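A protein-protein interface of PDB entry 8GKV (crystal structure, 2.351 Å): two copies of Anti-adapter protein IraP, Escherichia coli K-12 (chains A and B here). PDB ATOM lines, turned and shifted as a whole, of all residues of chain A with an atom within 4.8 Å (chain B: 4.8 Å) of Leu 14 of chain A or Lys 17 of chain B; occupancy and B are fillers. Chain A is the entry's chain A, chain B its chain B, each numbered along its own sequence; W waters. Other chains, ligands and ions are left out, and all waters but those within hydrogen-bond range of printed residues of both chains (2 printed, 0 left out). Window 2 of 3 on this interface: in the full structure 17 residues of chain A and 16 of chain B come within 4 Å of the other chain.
The side-chain hydroxyl (OG) of Ser 21 of chain A lies close to the side-chain carboxylate (OE2) of Glu 20 of chain B, 3.5 Å away.
NZ of Lys 17 of chain B lies within salt-bridge range of OE1 of Glu 20 of chain B (2.8 Å). The side-chain hydroxyl (OG) of Ser 21 of chain B sits at hydrogen-bond distance from the backbone carbonyl oxygen (O) of Lys 17 of chain B, at 3.4 Å.
Among the printed residues, merely in contact across the chains: Leu 11 of chain A with Leu 10 of chain B (3.7 Å), Leu 14 of chain A with Lys 17 of chain B (3.5 Å), Lys 17 of chain A with Leu 14 of chain B (3.7 Å), Lys 17 of chain A with Ser 21 of chain B (3.8 Å), Glu 18 of chain A with Lys 17 of chain B (3.7 Å), Ser 21 of chain A with Ser 21 of chain B (3.7 Å) and Lys 22 of chain A with Lys 17 of chain B (3.9 Å).
Leu 14 of chain A touches just one residue of chain B: Lys 17. Of the printed residues of chain A, Lys 17 of chain B touches Leu 14 (3.5 Å), Glu 18 (3.7 Å) and Lys 22 (3.9 Å). Of the printed residues of chain A, Leu 10 of chain B touches Leu 11 (3.7 Å). Printed residues of chain B within 4 Å of Glu 18 of chain A: Lys 17 (3.7 Å). Printed residues of chain B within 4 Å of Leu 11 of chain A: Leu 10. Of the printed residues of chain A, Glu 20 of chain B touches Ser 21 (3.2 Å). Gln 16 of chain A touches none of the printed residues of chain B. Lys 13 of chain B touches none of the printed residues of chain A.
Printed residues of chain A that touch a printed residue of chain B: Leu 11, Leu 14, Lys 17, Glu 18, Ser 21 and Lys 22. Hydrophobic or aromatic side chains of chain A that line the printed part of chain B: Leu 11 and Leu 14. Of the 10 printed residues of chain B, 5 touch a printed residue of chain A. Printed residues of chain B that touch a printed residue of chain A: Leu 10, Leu 14, Lys 17, Glu 20 and Ser 21. Among the printed residues, no Asp or Glu carboxylate lies within 4 Å of a Lys or Arg side-chain nitrogen of the other chain.
Leu 14 of chain A touches Lys 17 of chain B, and with the chains exchanged Lys 17 of chain A touches Leu 14 of chain B. Lys 17 of chain A touches Ser 21 of chain B, but with the chains exchanged Ser 21 of chain A does not touch Lys 17 of chain B (4.1 Å). Glu 18 of chain A touches Lys 17 of chain B, but with the chains exchanged Lys 17 of chain A does not touch Glu 18 of chain B (4.1 Å). Ser 21 of chain B touches its own counterpart, Ser 21 of chain A. Positions printed for both chains: 10, 13, 14, 15, 16, 17, 18 and 21. Of the 8 pairs that touch across the chains among the printed residues, 3 have their exchanged pair printed and touching as well.
Water W2 lies within hydrogen-bond range of the side-chain amino group (NZ) of Lys 17 of chain B, the side-chain amino group (NZ) of Lys 22 of chain A and the backbone carbonyl oxygen (O) of Glu 18 of chain A. Water W1 bridges OE2 of Glu 18 of chain A (2.5 Å) and NZ of Lys 13 of chain B (3.0 Å).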
ATOM      1  N   LEU A  10      12.737  19.469  21.426  1.00  0.00           N
ATOM      2  CA  LEU A  10      12.374  18.065  21.564  1.00  0.00           C
ATOM      3  C   LEU A  10      12.386  17.652  23.029  1.00  0.00           C
ATOM      4  O   LEU A  10      11.431  17.047  23.508  1.00  0.00           O
ATOM      5  CB  LEU A  10      13.323  17.170  20.765  1.00  0.00           C
ATOM      6  CG  LEU A  10      12.886  16.813  19.343  1.00  0.00           C
ATOM      7  CD1 LEU A  10      12.394  18.037  18.593  1.00  0.00           C
ATOM      8  CD2 LEU A  10      14.041  16.168  18.604  1.00  0.00           C
ATOM      9  N   LEU A  11      13.460  17.981  23.742  1.00  0.00           N
ATOM     10  CA  LEU A  11      13.565  17.601  25.146  1.00  0.00           C
ATOM     11  C   LEU A  11      12.437  18.223  25.960  1.00  0.00           C
ATOM     12  O   LEU A  11      11.840  17.561  26.810  1.00  0.00           O
ATOM     13  CB  LEU A  11      14.916  18.011  25.732  1.00  0.00           C
ATOM     14  CG  LEU A  11      15.208  17.420  27.116  1.00  0.00           C
ATOM     15  CD1 LEU A  11      15.368  15.905  27.054  1.00  0.00           C
ATOM     16  CD2 LEU A  11      16.442  18.047  27.733  1.00  0.00           C
ATOM     17  N   PHE A  12      12.140  19.495  25.701  1.00  0.00           N
ATOM     18  CA  PHE A  12      11.035  20.154  26.400  1.00  0.00           C
ATOM     19  C   PHE A  12       9.704  19.441  26.132  1.00  0.00           C
ATOM     20  O   PHE A  12       8.965  19.102  27.074  1.00  0.00           O
ATOM     21  CB  PHE A  12      10.938  21.624  25.985  1.00  0.00           C
ATOM     22  CG  PHE A  12      10.051  22.434  26.883  1.00  0.00           C
ATOM     23  CD1 PHE A  12      10.414  22.680  28.196  1.00  0.00           C
ATOM     24  CD2 PHE A  12       8.855  22.947  26.416  1.00  0.00           C
ATOM     25  CE1 PHE A  12       9.603  23.423  29.027  1.00  0.00           C
ATOM     26  CE2 PHE A  12       8.037  23.692  27.244  1.00  0.00           C
ATOM     27  CZ  PHE A  12       8.414  23.928  28.554  1.00  0.00           C
ATOM     28  N   LYS A  13       9.407  19.211  24.856  1.00  0.00           N
ATOM     29  CA  LYS A  13       8.206  18.465  24.475  1.00  0.00           C
ATOM     30  C   LYS A  13       8.154  17.140  25.235  1.00  0.00           C
ATOM     31  O   LYS A  13       7.131  16.778  25.826  1.00  0.00           O
ATOM     32  CB  LYS A  13       8.177  18.207  22.963  1.00  0.00           C
ATOM     33  CG  LYS A  13       6.894  18.644  22.254  1.00  0.00           C
ATOM     34  CD  LYS A  13       7.145  19.810  21.302  1.00  0.00           C
ATOM     35  CE  LYS A  13       5.850  20.334  20.692  1.00  0.00           C
ATOM     36  NZ  LYS A  13       5.792  20.112  19.219  1.00  0.00           N
ATOM     37  N   LEU A  14       9.280  16.434  25.229  1.00  0.00           N
ATOM     38  CA  LEU A  14       9.415  15.162  25.933  1.00  0.00           C
ATOM     39  C   LEU A  14       9.054  15.300  27.416  1.00  0.00           C
ATOM     40  O   LEU A  14       8.241  14.533  27.944  1.00  0.00           O
ATOM     41  CB  LEU A  14      10.844  14.645  25.786  1.00  0.00           C
ATOM     42  CG  LEU A  14      11.143  13.141  25.802  1.00  0.00           C
ATOM     43  CD1 LEU A  14      12.399  12.882  26.618  1.00  0.00           C
ATOM     44  CD2 LEU A  14       9.988  12.296  26.318  1.00  0.00           C
ATOM     45  N   ALA A  15       9.659  16.282  28.081  1.00  0.00           N
ATOM     46  CA  ALA A  15       9.377  16.542  29.495  1.00  0.00           C
ATOM     47  C   ALA A  15       7.873  16.744  29.715  1.00  0.00           C
ATOM     48  O   ALA A  15       7.256  16.111  30.602  1.00  0.00           O
ATOM     49  CB  ALA A  15      10.156  17.760  29.974  1.00  0.00           C
ATOM     50  N   GLN A  16       7.283  17.610  28.890  1.00  0.00           N
ATOM     51  CA  GLN A  16       5.838  17.840  28.944  1.00  0.00           C
ATOM     52  C   GLN A  16       5.044  16.539  28.835  1.00  0.00           C
ATOM     53  O   GLN A  16       4.212  16.238  29.697  1.00  0.00           O
ATOM     54  CB  GLN A  16       5.387  18.790  27.835  1.00  0.00           C
ATOM     55  CG  GLN A  16       5.734  20.249  28.061  1.00  0.00           C
ATOM     56  CD  GLN A  16       5.163  21.155  26.980  1.00  0.00           C
ATOM     57  OE1 GLN A  16       5.027  20.755  25.822  1.00  0.00           O
ATOM     58  NE2 GLN A  16       4.816  22.380  27.360  1.00  0.00           N
ATOM     59  N   LYS A  17       5.290  15.773  27.775  1.00  0.00           N
ATOM     60  CA  LYS A  17       4.541  14.534  27.568  1.00  0.00           C
ATOM     61  C   LYS A  17       4.734  13.573  28.735  1.00  0.00           C
ATOM     62  O   LYS A  17       3.797  12.879  29.134  1.00  0.00           O
ATOM     63  CB  LYS A  17       4.952  13.844  26.265  1.00  0.00           C
ATOM     64  CG  LYS A  17       4.760  14.672  25.001  1.00  0.00           C
ATOM     65  CD  LYS A  17       3.383  15.325  24.911  1.00  0.00           C
ATOM     66  CE  LYS A  17       2.254  14.304  24.873  1.00  0.00           C
ATOM     67  NZ  LYS A  17       1.004  14.897  24.312  1.00  0.00           N
ATOM     68  N   GLU A  18       5.943  13.531  29.286  1.00  0.00           N
ATOM     69  CA  GLU A  18       6.197  12.675  30.441  1.00  0.00           C
ATOM     70  C   GLU A  18       5.336  13.088  31.642  1.00  0.00           C
ATOM     71  O   GLU A  18       4.657  12.245  32.260  1.00  0.00           O
ATOM     72  CB  GLU A  18       7.686  12.695  30.793  1.00  0.00           C
ATOM     73  CG  GLU A  18       8.513  11.846  29.823  1.00  0.00           C
ATOM     74  CD  GLU A  18      10.012  11.937  30.051  1.00  0.00           C
ATOM     75  OE1 GLU A  18      10.439  12.672  30.965  1.00  0.00           O
ATOM     76  OE2 GLU A  18      10.765  11.270  29.308  1.00  0.00           O
ATOM     77  N   SER A  21       1.760  12.276  30.932  1.00  0.00           N
ATOM     78  CA  SER A  21       1.573  10.835  31.031  1.00  0.00           C
ATOM     79  C   SER A  21       1.452  10.401  32.485  1.00  0.00           C
ATOM     80  O   SER A  21       0.572   9.611  32.831  1.00  0.00           O
ATOM     81  CB  SER A  21       2.728  10.095  30.356  1.00  0.00           C
ATOM     82  OG  SER A  21       2.500   8.698  30.367  1.00  0.00           O
ATOM     83  N   LYS A  22       2.340  10.903  33.339  1.00  0.00           N
ATOM     84  CA  LYS A  22       2.247  10.568  34.763  1.00  0.00           C
ATOM     85  C   LYS A  22       0.891  11.003  35.354  1.00  0.00           C
ATOM     86  O   LYS A  22       0.232  10.231  36.081  1.00  0.00           O
ATOM     87  CB  LYS A  22       3.417  11.192  35.534  1.00  0.00           C
ATOM     88  CG  LYS A  22       4.771  10.555  35.206  1.00  0.00           C
ATOM     89  CD  LYS A  22       4.826   9.069  35.596  1.00  0.00           C
ATOM     90  CE  LYS A  22       5.421   8.197  34.489  1.00  0.00           C
ATOM     91  NZ  LYS A  22       4.589   8.160  33.247  1.00  0.00           N
ATOM     92  N   LEU B  10      15.920  10.890  21.142  1.00  0.00           N
ATOM     93  CA  LEU B  10      14.945  11.829  21.680  1.00  0.00           C
ATOM     94  C   LEU B  10      13.614  11.668  20.967  1.00  0.00           C
ATOM     95  O   LEU B  10      12.574  11.514  21.605  1.00  0.00           O
ATOM     96  CB  LEU B  10      15.427  13.272  21.539  1.00  0.00           C
ATOM     97  CG  LEU B  10      16.380  13.804  22.608  1.00  0.00           C
ATOM     98  CD1 LEU B  10      16.856  15.201  22.229  1.00  0.00           C
ATOM     99  CD2 LEU B  10      15.709  13.808  23.978  1.00  0.00           C
ATOM    100  N   LYS B  13      11.936   8.261  21.887  1.00  0.00           N
ATOM    101  CA  LYS B  13      11.363   8.380  23.227  1.00  0.00           C
ATOM    102  C   LYS B  13      10.077   9.202  23.184  1.00  0.00           C
ATOM    103  O   LYS B  13       9.037   8.785  23.709  1.00  0.00           O
ATOM    104  CB  LYS B  13      12.363   9.023  24.191  1.00  0.00           C
ATOM    105  CG  LYS B  13      13.120   8.033  25.056  1.00  0.00           C
ATOM    106  CD  LYS B  13      12.372   7.730  26.344  1.00  0.00           C
ATOM    107  CE  LYS B  13      13.175   6.794  27.237  1.00  0.00           C
ATOM    108  NZ  LYS B  13      12.447   6.450  28.490  1.00  0.00           N
ATOM    109  N   LEU B  14      10.157  10.361  22.536  1.00  0.00           N
ATOM    110  CA  LEU B  14       9.008  11.249  22.394  1.00  0.00           C
ATOM    111  C   LEU B  14       7.823  10.504  21.780  1.00  0.00           C
ATOM    112  O   LEU B  14       6.706  10.550  22.304  1.00  0.00           O
ATOM    113  CB  LEU B  14       9.361  12.455  21.526  1.00  0.00           C
ATOM    114  CG  LEU B  14       8.842  13.838  21.928  1.00  0.00           C
ATOM    115  CD1 LEU B  14       8.815  14.732  20.695  1.00  0.00           C
ATOM    116  CD2 LEU B  14       7.473  13.797  22.605  1.00  0.00           C
ATOM    117  N   ALA B  15       8.077   9.814  20.668  1.00  0.00           N
ATOM    118  CA  ALA B  15       7.037   9.035  19.998  1.00  0.00           C
ATOM    119  C   ALA B  15       6.390   8.052  20.975  1.00  0.00           C
ATOM    120  O   ALA B  15       5.148   7.976  21.094  1.00  0.00           O
ATOM    121  CB  ALA B  15       7.613   8.291  18.804  1.00  0.00           C
ATOM    122  N   GLN B  16       7.241   7.313  21.687  1.00  0.00           N
ATOM    123  CA  GLN B  16       6.755   6.359  22.680  1.00  0.00           C
ATOM    124  C   GLN B  16       5.852   7.045  23.715  1.00  0.00           C
ATOM    125  O   GLN B  16       4.741   6.574  23.992  1.00  0.00           O
ATOM    126  CB  GLN B  16       7.926   5.656  23.375  1.00  0.00           C
ATOM    127  CG  GLN B  16       8.873   4.935  22.419  1.00  0.00           C
ATOM    128  CD  GLN B  16       9.471   3.671  23.011  1.00  0.00           C
ATOM    129  OE1 GLN B  16       9.374   2.593  22.422  1.00  0.00           O
ATOM    130  NE2 GLN B  16      10.111   3.798  24.169  1.00  0.00           N
ATOM    131  N   LYS B  17       6.316   8.165  24.266  1.00  0.00           N
ATOM    132  CA  LYS B  17       5.519   8.898  25.254  1.00  0.00           C
ATOM    133  C   LYS B  17       4.187   9.380  24.676  1.00  0.00           C
ATOM    134  O   LYS B  17       3.157   9.303  25.347  1.00  0.00           O
ATOM    135  CB  LYS B  17       6.296  10.096  25.809  1.00  0.00           C
ATOM    136  CG  LYS B  17       7.600   9.747  26.510  1.00  0.00           C
ATOM    137  CD  LYS B  17       7.438   8.670  27.577  1.00  0.00           C
ATOM    138  CE  LYS B  17       6.396   9.047  28.616  1.00  0.00           C
ATOM    139  NZ  LYS B  17       6.527   8.224  29.851  1.00  0.00           N
ATOM    140  N   GLU B  18       4.204   9.883  23.444  1.00  0.00           N
ATOM    141  CA  GLU B  18       2.969  10.326  22.801  1.00  0.00           C
ATOM    142  C   GLU B  18       1.970   9.172  22.668  1.00  0.00           C
ATOM    143  O   GLU B  18       0.788   9.310  23.027  1.00  0.00           O
ATOM    144  CB  GLU B  18       3.273  10.937  21.432  1.00  0.00           C
ATOM    145  CG  GLU B  18       3.640  12.417  21.502  1.00  0.00           C
ATOM    146  CD  GLU B  18       4.355  12.927  20.254  1.00  0.00           C
ATOM    147  OE1 GLU B  18       4.716  12.104  19.384  1.00  0.00           O
ATOM    148  OE2 GLU B  18       4.559  14.157  20.144  1.00  0.00           O
ATOM    149  N   GLU B  19       2.442   8.034  22.164  1.00  0.00           N
ATOM    150  CA  GLU B  19       1.580   6.852  22.072  1.00  0.00           C
ATOM    151  C   GLU B  19       1.035   6.428  23.447  1.00  0.00           C
ATOM    152  O   GLU B  19      -0.172   6.145  23.605  1.00  0.00           O
ATOM    153  CB  GLU B  19       2.341   5.694  21.420  1.00  0.00           C
ATOM    154  CG  GLU B  19       2.451   5.809  19.906  1.00  0.00           C
ATOM    155  CD  GLU B  19       1.092   5.856  19.221  1.00  0.00           C
ATOM    156  OE1 GLU B  19       0.193   5.089  19.630  1.00  0.00           O
ATOM    157  OE2 GLU B  19       0.919   6.665  18.284  1.00  0.00           O
ATOM    158  N   GLU B  20       1.917   6.393  24.445  1.00  0.00           N
ATOM    159  CA  GLU B  20       1.502   6.079  25.811  1.00  0.00           C
ATOM    160  C   GLU B  20       0.389   7.023  26.279  1.00  0.00           C
ATOM    161  O   GLU B  20      -0.653   6.576  26.774  1.00  0.00           O
ATOM    162  CB  GLU B  20       2.696   6.150  26.767  1.00  0.00           C
ATOM    163  CG  GLU B  20       2.342   5.892  28.222  1.00  0.00           C
ATOM    164  CD  GLU B  20       3.560   5.914  29.126  1.00  0.00           C
ATOM    165  OE1 GLU B  20       4.600   6.466  28.710  1.00  0.00           O
ATOM    166  OE2 GLU B  20       3.480   5.378  30.252  1.00  0.00           O
ATOM    167  N   SER B  21       0.611   8.326  26.121  1.00  0.00           N
ATOM    168  CA  SER B  21      -0.390   9.318  26.504  1.00  0.00           C
ATOM    169  C   SER B  21      -1.709   9.085  25.769  1.00  0.00           C
ATOM    170  O   SER B  21      -2.778   9.165  26.374  1.00  0.00           O
ATOM    171  CB  SER B  21       0.118  10.739  26.233  1.00  0.00           C
ATOM    172  OG  SER B  21       1.013  11.161  27.247  1.00  0.00           O
HETATM  173  O   HOH W   1      10.686   8.723  29.402  1.00  0.00           O
HETATM  174  O   HOH W   2       6.351   9.575  31.888  1.00  0.00           O
